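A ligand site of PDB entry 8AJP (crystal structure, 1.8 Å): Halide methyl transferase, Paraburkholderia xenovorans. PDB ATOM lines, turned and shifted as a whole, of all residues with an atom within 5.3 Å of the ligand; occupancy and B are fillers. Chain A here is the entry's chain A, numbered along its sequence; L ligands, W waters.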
ATOM      1  N   PRO A  17      -7.586 -14.944  -5.258  1.00  0.00           N
ATOM      2  CA  PRO A  17      -8.963 -14.463  -5.033  1.00  0.00           C
ATOM      3  C   PRO A  17      -9.039 -12.978  -4.710  1.00  0.00           C
ATOM      4  O   PRO A  17     -10.148 -12.428  -4.696  1.00  0.00           O
ATOM      5  CB  PRO A  17      -9.445 -15.308  -3.830  1.00  0.00           C
ATOM      6  CG  PRO A  17      -8.430 -16.414  -3.694  1.00  0.00           C
ATOM      7  CD  PRO A  17      -7.146 -15.852  -4.198  1.00  0.00           C
ATOM      8  N   TRP A  23     -12.439 -14.176 -10.055  1.00  0.00           N
ATOM      9  CA  TRP A  23     -13.874 -14.442 -10.027  1.00  0.00           C
ATOM     10  C   TRP A  23     -14.483 -14.384 -11.417  1.00  0.00           C
ATOM     11  O   TRP A  23     -15.411 -15.141 -11.716  1.00  0.00           O
ATOM     12  CB  TRP A  23     -14.519 -13.465  -9.046  1.00  0.00           C
ATOM     13  CG  TRP A  23     -13.930 -13.669  -7.663  1.00  0.00           C
ATOM     14  CD1 TRP A  23     -12.928 -12.967  -7.074  1.00  0.00           C
ATOM     15  CD2 TRP A  23     -14.293 -14.709  -6.733  1.00  0.00           C
ATOM     16  NE1 TRP A  23     -12.645 -13.484  -5.815  1.00  0.00           N
ATOM     17  CE2 TRP A  23     -13.482 -14.554  -5.594  1.00  0.00           C
ATOM     18  CE3 TRP A  23     -15.246 -15.728  -6.762  1.00  0.00           C
ATOM     19  CZ2 TRP A  23     -13.590 -15.394  -4.485  1.00  0.00           C
ATOM     20  CZ3 TRP A  23     -15.340 -16.572  -5.654  1.00  0.00           C
ATOM     21  CH2 TRP A  23     -14.511 -16.397  -4.539  1.00  0.00           C
ATOM     22  N   PHE A  27     -17.178 -17.330 -12.938  1.00  0.00           N
ATOM     23  CA  PHE A  27     -18.455 -16.985 -13.534  1.00  0.00           C
ATOM     24  C   PHE A  27     -18.458 -17.313 -15.024  1.00  0.00           C
ATOM     25  O   PHE A  27     -19.390 -17.944 -15.535  1.00  0.00           O
ATOM     26  CB  PHE A  27     -18.754 -15.501 -13.324  1.00  0.00           C
ATOM     27  CG  PHE A  27     -19.388 -15.196 -11.997  1.00  0.00           C
ATOM     28  CD1 PHE A  27     -18.621 -14.729 -10.955  1.00  0.00           C
ATOM     29  CD2 PHE A  27     -20.749 -15.389 -11.805  1.00  0.00           C
ATOM     30  CE1 PHE A  27     -19.181 -14.466  -9.735  1.00  0.00           C
ATOM     31  CE2 PHE A  27     -21.329 -15.115 -10.581  1.00  0.00           C
ATOM     32  CZ  PHE A  27     -20.545 -14.638  -9.536  1.00  0.00           C
ATOM     33  N   TRP A  34     -20.977 -21.845  -5.134  1.00  0.00           N
ATOM     34  CA  TRP A  34     -21.651 -21.113  -4.067  1.00  0.00           C
ATOM     35  C   TRP A  34     -23.057 -20.677  -4.436  1.00  0.00           C
ATOM     36  O   TRP A  34     -23.776 -20.171  -3.572  1.00  0.00           O
ATOM     37  CB  TRP A  34     -20.817 -19.877  -3.716  1.00  0.00           C
ATOM     38  CG  TRP A  34     -20.730 -18.955  -4.893  1.00  0.00           C
ATOM     39  CD1 TRP A  34     -21.671 -18.051  -5.295  1.00  0.00           C
ATOM     40  CD2 TRP A  34     -19.686 -18.920  -5.885  1.00  0.00           C
ATOM     41  NE1 TRP A  34     -21.258 -17.430  -6.447  1.00  0.00           N
ATOM     42  CE2 TRP A  34     -20.046 -17.932  -6.832  1.00  0.00           C
ATOM     43  CE3 TRP A  34     -18.472 -19.591  -6.041  1.00  0.00           C
ATOM     44  CZ2 TRP A  34     -19.242 -17.614  -7.926  1.00  0.00           C
ATOM     45  CZ3 TRP A  34     -17.668 -19.274  -7.136  1.00  0.00           C
ATOM     46  CH2 TRP A  34     -18.064 -18.294  -8.055  1.00  0.00           C
ATOM     47  N   ASP A  35     -23.451 -20.790  -5.698  1.00  0.00           N
ATOM     48  CA  ASP A  35     -24.630 -20.068  -6.145  1.00  0.00           C
ATOM     49  C   ASP A  35     -25.899 -20.809  -5.711  1.00  0.00           C
ATOM     50  O   ASP A  35     -26.046 -22.007  -5.956  1.00  0.00           O
ATOM     51  CB  ASP A  35     -24.601 -19.860  -7.657  1.00  0.00           C
ATOM     52  CG  ASP A  35     -25.584 -18.809  -8.105  1.00  0.00           C
ATOM     53  OD1 ASP A  35     -25.206 -17.604  -8.221  1.00  0.00           O
ATOM     54  OD2 ASP A  35     -26.750 -19.183  -8.305  1.00  0.00           O
ATOM     55  N   GLN A  36     -26.788 -20.082  -5.042  1.00  0.00           N
ATOM     56  CA  GLN A  36     -27.995 -20.639  -4.472  1.00  0.00           C
ATOM     57  C   GLN A  36     -29.094 -20.869  -5.507  1.00  0.00           C
ATOM     58  O   GLN A  36     -30.027 -21.630  -5.249  1.00  0.00           O
ATOM     59  CB  GLN A  36     -28.527 -19.696  -3.383  1.00  0.00           C
ATOM     60  CG  GLN A  36     -29.730 -20.178  -2.608  1.00  0.00           C
ATOM     61  CD  GLN A  36     -29.367 -21.094  -1.447  1.00  0.00           C
ATOM     62  OE1 GLN A  36     -28.200 -21.177  -1.051  1.00  0.00           O
ATOM     63  NE2 GLN A  36     -30.359 -21.785  -0.904  1.00  0.00           N
ATOM     64  N   PRO A  58     -22.420  -6.694  -0.076  1.00  0.00           N
ATOM     65  CA  PRO A  58     -21.071  -6.769  -0.663  1.00  0.00           C
ATOM     66  C   PRO A  58     -20.800  -8.133  -1.277  1.00  0.00           C
ATOM     67  O   PRO A  58     -21.299  -9.164  -0.823  1.00  0.00           O
ATOM     68  CB  PRO A  58     -20.153  -6.537   0.537  1.00  0.00           C
ATOM     69  CG  PRO A  58     -20.924  -7.073   1.686  1.00  0.00           C
ATOM     70  CD  PRO A  58     -22.369  -6.763   1.399  1.00  0.00           C
ATOM     71  N   GLY A  59     -20.006  -8.127  -2.349  1.00  0.00           N
ATOM     72  CA  GLY A  59     -19.684  -9.340  -3.059  1.00  0.00           C
ATOM     73  C   GLY A  59     -20.935 -10.043  -3.540  1.00  0.00           C
ATOM     74  O   GLY A  59     -21.076 -11.262  -3.390  1.00  0.00           O
ATOM     75  N   CYS A  60     -21.852  -9.280  -4.156  1.00  0.00           N
ATOM     76  CA  CYS A  60     -23.221  -9.759  -4.333  1.00  0.00           C
ATOM     77  C   CYS A  60     -23.352 -10.898  -5.327  1.00  0.00           C
ATOM     78  O   CYS A  60     -24.405 -11.553  -5.343  1.00  0.00           O
ATOM     79  CB  CYS A  60     -24.122  -8.602  -4.787  1.00  0.00           C
ATOM     80  SG  CYS A  60     -23.633  -7.932  -6.405  1.00  0.00           S
ATOM     81  N   GLY A  61     -22.351 -11.148  -6.172  1.00  0.00           N
ATOM     82  CA  GLY A  61     -22.539 -12.180  -7.195  1.00  0.00           C
ATOM     83  C   GLY A  61     -23.808 -11.947  -8.008  1.00  0.00           C
ATOM     84  O   GLY A  61     -24.107 -10.831  -8.405  1.00  0.00           O
ATOM     85  N   SER A  62     -24.606 -13.018  -8.218  1.00  0.00           N
ATOM     86  CA  SER A  62     -25.812 -12.925  -9.045  1.00  0.00           C
ATOM     87  C   SER A  62     -26.842 -11.971  -8.451  1.00  0.00           C
ATOM     88  O   SER A  62     -27.751 -11.543  -9.168  1.00  0.00           O
ATOM     89  CB  SER A  62     -26.474 -14.305  -9.206  1.00  0.00           C
ATOM     90  OG  SER A  62     -25.594 -15.247  -9.799  1.00  0.00           O
ATOM     91  N   GLU A  65     -30.775 -11.753  -3.970  1.00  0.00           N
ATOM     92  CA  GLU A  65     -31.333 -11.069  -2.820  1.00  0.00           C
ATOM     93  C   GLU A  65     -31.645  -9.606  -3.123  1.00  0.00           C
ATOM     94  O   GLU A  65     -32.540  -9.033  -2.495  1.00  0.00           O
ATOM     95  CB  GLU A  65     -30.358 -11.164  -1.643  1.00  0.00           C
ATOM     96  CG  GLU A  65     -30.213 -12.575  -1.106  1.00  0.00           C
ATOM     97  CD  GLU A  65     -29.095 -13.349  -1.774  1.00  0.00           C
ATOM     98  OE1 GLU A  65     -28.620 -12.920  -2.851  1.00  0.00           O
ATOM     99  OE2 GLU A  65     -28.695 -14.402  -1.206  1.00  0.00           O
ATOM    100  N   ILE A  79     -22.966  -4.694  -4.529  1.00  0.00           N
ATOM    101  CA  ILE A  79     -21.698  -4.370  -5.176  1.00  0.00           C
ATOM    102  C   ILE A  79     -20.886  -5.639  -5.342  1.00  0.00           C
ATOM    103  O   ILE A  79     -20.938  -6.563  -4.523  1.00  0.00           O
ATOM    104  CB  ILE A  79     -20.882  -3.305  -4.398  1.00  0.00           C
ATOM    105  CG1 ILE A  79     -20.513  -3.787  -2.987  1.00  0.00           C
ATOM    106  CG2 ILE A  79     -21.592  -1.960  -4.414  1.00  0.00           C
ATOM    107  CD1 ILE A  79     -19.368  -3.009  -2.337  1.00  0.00           C
ATOM    108  N   ASP A  80     -20.101  -5.672  -6.427  1.00  0.00           N
ATOM    109  CA  ASP A  80     -19.206  -6.781  -6.696  1.00  0.00           C
ATOM    110  C   ASP A  80     -18.115  -6.225  -7.587  1.00  0.00           C
ATOM    111  O   ASP A  80     -18.401  -5.381  -8.432  1.00  0.00           O
ATOM    112  CB  ASP A  80     -19.929  -7.930  -7.405  1.00  0.00           C
ATOM    113  CG  ASP A  80     -19.178  -9.207  -7.280  1.00  0.00           C
ATOM    114  OD1 ASP A  80     -18.046  -9.260  -7.803  1.00  0.00           O
ATOM    115  OD2 ASP A  80     -19.694 -10.130  -6.611  1.00  0.00           O
ATOM    116  N   PHE A  81     -16.849  -6.557  -7.292  1.00  0.00           N
ATOM    117  CA  PHE A  81     -15.706  -5.931  -8.021  1.00  0.00           C
ATOM    118  C   PHE A  81     -15.415  -6.709  -9.314  1.00  0.00           C
ATOM    119  O   PHE A  81     -14.583  -6.299 -10.092  1.00  0.00           O
ATOM    120  CB  PHE A  81     -14.487  -5.820  -7.105  1.00  0.00           C
ATOM    121  CG  PHE A  81     -13.668  -7.054  -6.817  1.00  0.00           C
ATOM    122  CD1 PHE A  81     -14.189  -8.334  -6.920  1.00  0.00           C
ATOM    123  CD2 PHE A  81     -12.359  -6.928  -6.389  1.00  0.00           C
ATOM    124  CE1 PHE A  81     -13.416  -9.448  -6.636  1.00  0.00           C
ATOM    125  CE2 PHE A  81     -11.592  -8.037  -6.093  1.00  0.00           C
ATOM    126  CZ  PHE A  81     -12.123  -9.295  -6.210  1.00  0.00           C
ATOM    127  N   SER A  82     -16.128  -7.792  -9.505  1.00  0.00           N
ATOM    128  CA  SER A  82     -16.012  -8.659 -10.686  1.00  0.00           C
ATOM    129  C   SER A  82     -16.924  -8.225 -11.822  1.00  0.00           C
ATOM    130  O   SER A  82     -18.149  -8.254 -11.667  1.00  0.00           O
ATOM    131  CB  SER A  82     -16.369 -10.081 -10.304  1.00  0.00           C
ATOM    132  OG  SER A  82     -16.365 -10.899 -11.483  1.00  0.00           O
ATOM    133  N   ALA A  85     -19.334 -11.045 -12.471  1.00  0.00           N
ATOM    134  CA  ALA A  85     -20.365 -11.095 -11.442  1.00  0.00           C
ATOM    135  C   ALA A  85     -21.424 -10.036 -11.679  1.00  0.00           C
ATOM    136  O   ALA A  85     -22.627 -10.311 -11.605  1.00  0.00           O
ATOM    137  CB  ALA A  85     -19.731 -10.936 -10.053  1.00  0.00           C
ATOM    138  N   ALA A 104     -17.924  -2.504  -7.862  1.00  0.00           N
ATOM    139  CA  ALA A 104     -17.185  -1.731  -6.867  1.00  0.00           C
ATOM    140  C   ALA A 104     -16.458  -2.664  -5.913  1.00  0.00           C
ATOM    141  O   ALA A 104     -16.906  -3.788  -5.646  1.00  0.00           O
ATOM    142  CB  ALA A 104     -18.103  -0.804  -6.069  1.00  0.00           C
ATOM    143  N   ASP A 105     -15.308  -2.185  -5.446  1.00  0.00           N
ATOM    144  CA  ASP A 105     -14.524  -2.762  -4.361  1.00  0.00           C
ATOM    145  C   ASP A 105     -15.184  -2.478  -3.021  1.00  0.00           C
ATOM    146  O   ASP A 105     -15.269  -1.313  -2.604  1.00  0.00           O
ATOM    147  CB  ASP A 105     -13.134  -2.123  -4.330  1.00  0.00           C
ATOM    148  CG  ASP A 105     -12.215  -2.766  -3.305  1.00  0.00           C
ATOM    149  OD1 ASP A 105     -12.624  -3.733  -2.626  1.00  0.00           O
ATOM    150  OD2 ASP A 105     -11.174  -2.147  -3.037  1.00  0.00           O
ATOM    151  N   PHE A 106     -15.582  -3.533  -2.318  1.00  0.00           N
ATOM    152  CA  PHE A 106     -16.173  -3.363  -0.982  1.00  0.00           C
ATOM    153  C   PHE A 106     -15.287  -2.532  -0.058  1.00  0.00           C
ATOM    154  O   PHE A 106     -15.784  -1.776   0.790  1.00  0.00           O
ATOM    155  CB  PHE A 106     -16.403  -4.747  -0.373  1.00  0.00           C
ATOM    156  CG  PHE A 106     -16.666  -4.733   1.121  1.00  0.00           C
ATOM    157  CD1 PHE A 106     -17.823  -4.172   1.633  1.00  0.00           C
ATOM    158  CD2 PHE A 106     -15.774  -5.332   1.991  1.00  0.00           C
ATOM    159  CE1 PHE A 106     -18.071  -4.197   3.009  1.00  0.00           C
ATOM    160  CE2 PHE A 106     -16.008  -5.360   3.367  1.00  0.00           C
ATOM    161  CZ  PHE A 106     -17.162  -4.783   3.873  1.00  0.00           C
ATOM    162  N   PHE A 107     -13.982  -2.677  -0.163  1.00  0.00           N
ATOM    163  CA  PHE A 107     -13.089  -1.977   0.759  1.00  0.00           C
ATOM    164  C   PHE A 107     -12.876  -0.516   0.386  1.00  0.00           C
ATOM    165  O   PHE A 107     -12.276   0.225   1.188  1.00  0.00           O
ATOM    166  CB  PHE A 107     -11.768  -2.730   0.811  1.00  0.00           C
ATOM    167  CG  PHE A 107     -11.919  -4.087   1.420  1.00  0.00           C
ATOM    168  CD1 PHE A 107     -12.090  -4.221   2.793  1.00  0.00           C
ATOM    169  CD2 PHE A 107     -11.946  -5.221   0.631  1.00  0.00           C
ATOM    170  CE1 PHE A 107     -12.248  -5.475   3.374  1.00  0.00           C
ATOM    171  CE2 PHE A 107     -12.112  -6.477   1.200  1.00  0.00           C
ATOM    172  CZ  PHE A 107     -12.244  -6.599   2.578  1.00  0.00           C
ATOM    173  N   ARG A 121     -23.392 -13.136   2.403  1.00  0.00           N
ATOM    174  CA  ARG A 121     -23.503 -14.521   1.961  1.00  0.00           C
ATOM    175  C   ARG A 121     -22.323 -14.839   1.078  1.00  0.00           C
ATOM    176  O   ARG A 121     -22.116 -14.161   0.065  1.00  0.00           O
ATOM    177  CB  ARG A 121     -24.808 -14.825   1.200  1.00  0.00           C
ATOM    178  CG  ARG A 121     -24.955 -16.311   0.924  1.00  0.00           C
ATOM    179  CD  ARG A 121     -26.129 -16.669  -0.020  1.00  0.00           C
ATOM    180  NE  ARG A 121     -26.176 -18.111  -0.226  1.00  0.00           N
ATOM    181  CZ  ARG A 121     -25.469 -18.755  -1.147  1.00  0.00           C
ATOM    182  NH1 ARG A 121     -24.658 -18.077  -1.953  1.00  0.00           N
ATOM    183  NH2 ARG A 121     -25.569 -20.067  -1.249  1.00  0.00           N
ATOM    184  N   ALA A 122     -21.562 -15.866   1.454  1.00  0.00           N
ATOM    185  CA  ALA A 122     -20.464 -16.372   0.643  1.00  0.00           C
ATOM    186  C   ALA A 122     -19.487 -15.252   0.242  1.00  0.00           C
ATOM    187  O   ALA A 122     -18.845 -15.317  -0.805  1.00  0.00           O
ATOM    188  CB  ALA A 122     -21.000 -17.099  -0.584  1.00  0.00           C
ATOM    189  N   PHE A 123     -19.372 -14.222   1.073  1.00  0.00           N
ATOM    190  CA  PHE A 123     -18.429 -13.128   0.842  1.00  0.00           C
ATOM    191  C   PHE A 123     -17.227 -13.193   1.772  1.00  0.00           C
ATOM    192  O   PHE A 123     -16.082 -13.234   1.317  1.00  0.00           O
ATOM    193  CB  PHE A 123     -19.121 -11.769   0.978  1.00  0.00           C
ATOM    194  CG  PHE A 123     -18.175 -10.613   0.831  1.00  0.00           C
ATOM    195  CD1 PHE A 123     -17.395 -10.495  -0.309  1.00  0.00           C
ATOM    196  CD2 PHE A 123     -18.041  -9.658   1.827  1.00  0.00           C
ATOM    197  CE1 PHE A 123     -16.480  -9.451  -0.442  1.00  0.00           C
ATOM    198  CE2 PHE A 123     -17.136  -8.598   1.699  1.00  0.00           C
ATOM    199  CZ  PHE A 123     -16.355  -8.501   0.552  1.00  0.00           C
ATOM    200  N   ALA A 126     -15.148 -15.787   0.674  1.00  0.00           N
ATOM    201  CA  ALA A 126     -14.444 -15.559  -0.579  1.00  0.00           C
ATOM    202  C   ALA A 126     -13.108 -14.881  -0.357  1.00  0.00           C
ATOM    203  O   ALA A 126     -12.259 -14.890  -1.264  1.00  0.00           O
ATOM    204  CB  ALA A 126     -15.293 -14.688  -1.516  1.00  0.00           C
ATOM    205  N   LEU A 127     -12.911 -14.261   0.814  1.00  0.00           N
ATOM    206  CA  LEU A 127     -11.742 -13.416   1.023  1.00  0.00           C
ATOM    207  C   LEU A 127     -10.544 -14.249   1.466  1.00  0.00           C
ATOM    208  O   LEU A 127     -10.681 -15.108   2.336  1.00  0.00           O
ATOM    209  CB  LEU A 127     -12.030 -12.353   2.085  1.00  0.00           C
ATOM    210  CG  LEU A 127     -13.133 -11.344   1.756  1.00  0.00           C
ATOM    211  CD1 LEU A 127     -13.376 -10.425   2.940  1.00  0.00           C
ATOM    212  CD2 LEU A 127     -12.793 -10.534   0.485  1.00  0.00           C
HETATM  213  N1  LIG L   1     -22.609 -13.290  -2.453  1.00  0.00           N
HETATM  214  C1  LIG L   1     -22.836 -13.956  -3.735  1.00  0.00           C
HETATM  215  C2  LIG L   1     -21.530 -14.298  -4.433  1.00  0.00           C
HETATM  216  C3  LIG L   1     -20.477 -15.012  -3.607  1.00  0.00           C
HETATM  217  S1  LIG L   1     -19.014 -15.402  -4.612  1.00  0.00           S
HETATM  218  C4  LIG L   1     -23.691 -15.206  -3.490  1.00  0.00           C
HETATM  219  O1  LIG L   1     -24.089 -15.893  -4.436  1.00  0.00           O
HETATM  220  O2  LIG L   1     -23.991 -15.518  -2.338  1.00  0.00           O
HETATM  221  C5  LIG L   1     -17.927 -14.102  -3.969  1.00  0.00           C
HETATM  222  C6  LIG L   1     -18.128 -12.803  -4.703  1.00  0.00           C
HETATM  223  O3  LIG L   1     -17.539 -11.736  -3.973  1.00  0.00           O
HETATM  224  C7  LIG L   1     -17.561 -12.730  -6.149  1.00  0.00           C
HETATM  225  O4  LIG L   1     -18.590 -12.351  -7.043  1.00  0.00           O
HETATM  226  C8  LIG L   1     -16.438 -11.701  -6.112  1.00  0.00           C
HETATM  227  O5  LIG L   1     -16.293 -10.942  -7.278  1.00  0.00           O
HETATM  228  C9  LIG L   1     -16.826 -10.858  -4.873  1.00  0.00           C
HETATM  229  N2  LIG L   1     -15.744 -10.141  -4.203  1.00  0.00           N
HETATM  230  C10 LIG L   1     -14.573 -10.624  -3.665  1.00  0.00           C
HETATM  231  N3  LIG L   1     -13.889  -9.577  -3.150  1.00  0.00           N
HETATM  232  C11 LIG L   1     -14.611  -8.451  -3.324  1.00  0.00           C
HETATM  233  C12 LIG L   1     -14.380  -7.116  -3.021  1.00  0.00           C
HETATM  234  N4  LIG L   1     -13.265  -6.759  -2.396  1.00  0.00           N
HETATM  235  N5  LIG L   1     -15.331  -6.174  -3.326  1.00  0.00           N
HETATM  236  C13 LIG L   1     -16.485  -6.537  -3.975  1.00  0.00           C
HETATM  237  N6  LIG L   1     -16.698  -7.856  -4.293  1.00  0.00           N
HETATM  238  C14 LIG L   1     -15.790  -8.794  -3.967  1.00  0.00           C
HETATM  239  O   HOH W   1     -11.243 -10.731  -2.614  1.00  0.00           O
HETATM  240  O   HOH W   2     -26.807 -13.901  -4.907  1.00  0.00           O
HETATM  241  O   HOH W   3     -26.420 -17.267  -4.665  1.00  0.00           O
HETATM  242  O   HOH W   4     -24.711 -12.000  -1.242  1.00  0.00           O
HETATM  243  O   HOH W   5     -23.607 -15.586  -7.167  1.00  0.00           O
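A nitrogen (N6) of the ligand sits at hydrogen-bond distance from the backbone NH (N) of Phe 81 (3.3 Å).
The backbone carbonyl oxygen of Arg 121 lies within hydrogen-bond range of a nitrogen (N1) of the ligand, at 2.7 Å.
NH1 of Arg 121 is in salt-bridge range of O2 of the ligand (2.7 Å).
The indole nitrogen (NE1) of Trp 34 lies close to a sulfur (S1) of the ligand (3.5 Å).
OD1 of Asp 80 is in hydrogen-bond range of O5 of the ligand (2.5 Å).
OD1 of Asp 105 lies within hydrogen-bond range of N4 of the ligand.
N of Phe 106 sits at hydrogen-bond distance from N5 of the ligand (2.8 Å).
The backbone carbonyl oxygen (O) of Gly 59 is in hydrogen-bond range of a nitrogen (N1) of the ligand, 2.7 Å away.
The backbone carbonyl oxygen of Ala 104 is in hydrogen-bond range of the backbone NH of Phe 81, at 3.2 Å.
The backbone carbonyl oxygen of Pro 17 sits at hydrogen-bond distance from the indole nitrogen of Trp 23 (2.9 Å).
The side-chain hydroxyl (OG) of Ser 82 sits at hydrogen-bond distance from the backbone NH (N) of Ala 85, at 3.1 Å.
The side-chain carboxylate (OD2) of Asp 80 lies within hydrogen-bond range of the backbone NH (N) of Cys 60 (3.4 Å).
The backbone carbonyl oxygen of Asp 80 is in hydrogen-bond range of the backbone NH of Ala 104 (3.0 Å).
The side-chain carboxylate of Asp 105 lies within hydrogen-bond range of the backbone NH of Phe 107.
NH1 of Arg 121 is in hydrogen-bond range of O of Trp 34 (2.8 Å).
NH2 of Arg 121 is in hydrogen-bond range of OE1 of Gln 36, 2.9 Å away.
Merely in contact with the ligand: Trp 23, Phe 27, Cys 60, Gly 61, Ser 82, Ala 85, Ala 104, Phe 107, Ala 122, Phe 123, Ala 126 and Leu 127.
Hydrophobic or aromatic side chains within 4 Å of the ligand: Trp 23, Phe 27, Trp 34, Phe 81, Ala 85, Phe 106, Phe 107, Ala 122, Phe 123, Ala 126 and Leu 127.
Of the 26 residues printed, 19 come within 4 Å of the ligand.
Water W3 lies within hydrogen-bond range of an oxygen (O1) of the ligand (2.7 Å), the backbone NH of Gln 36 (2.9 Å) and the guanidinium group of Arg 121 (3.3 Å).
Water W5 lies within hydrogen-bond range of OD1 of Asp 35 (2.8 Å), O1 of the ligand (2.8 Å), N of Ser 62 (2.9 Å) and NE1 of Trp 34 (3.1 Å).
Water W1 bridges the backbone carbonyl oxygen of Pro 17 (2.9 Å) and a nitrogen (N3) of the ligand (2.9 Å).
Water W2 lies within hydrogen-bond range of OE1 of Glu 65 (2.9 Å), O of Cys 60 (3.4 Å) and O1 of the ligand (3.4 Å).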
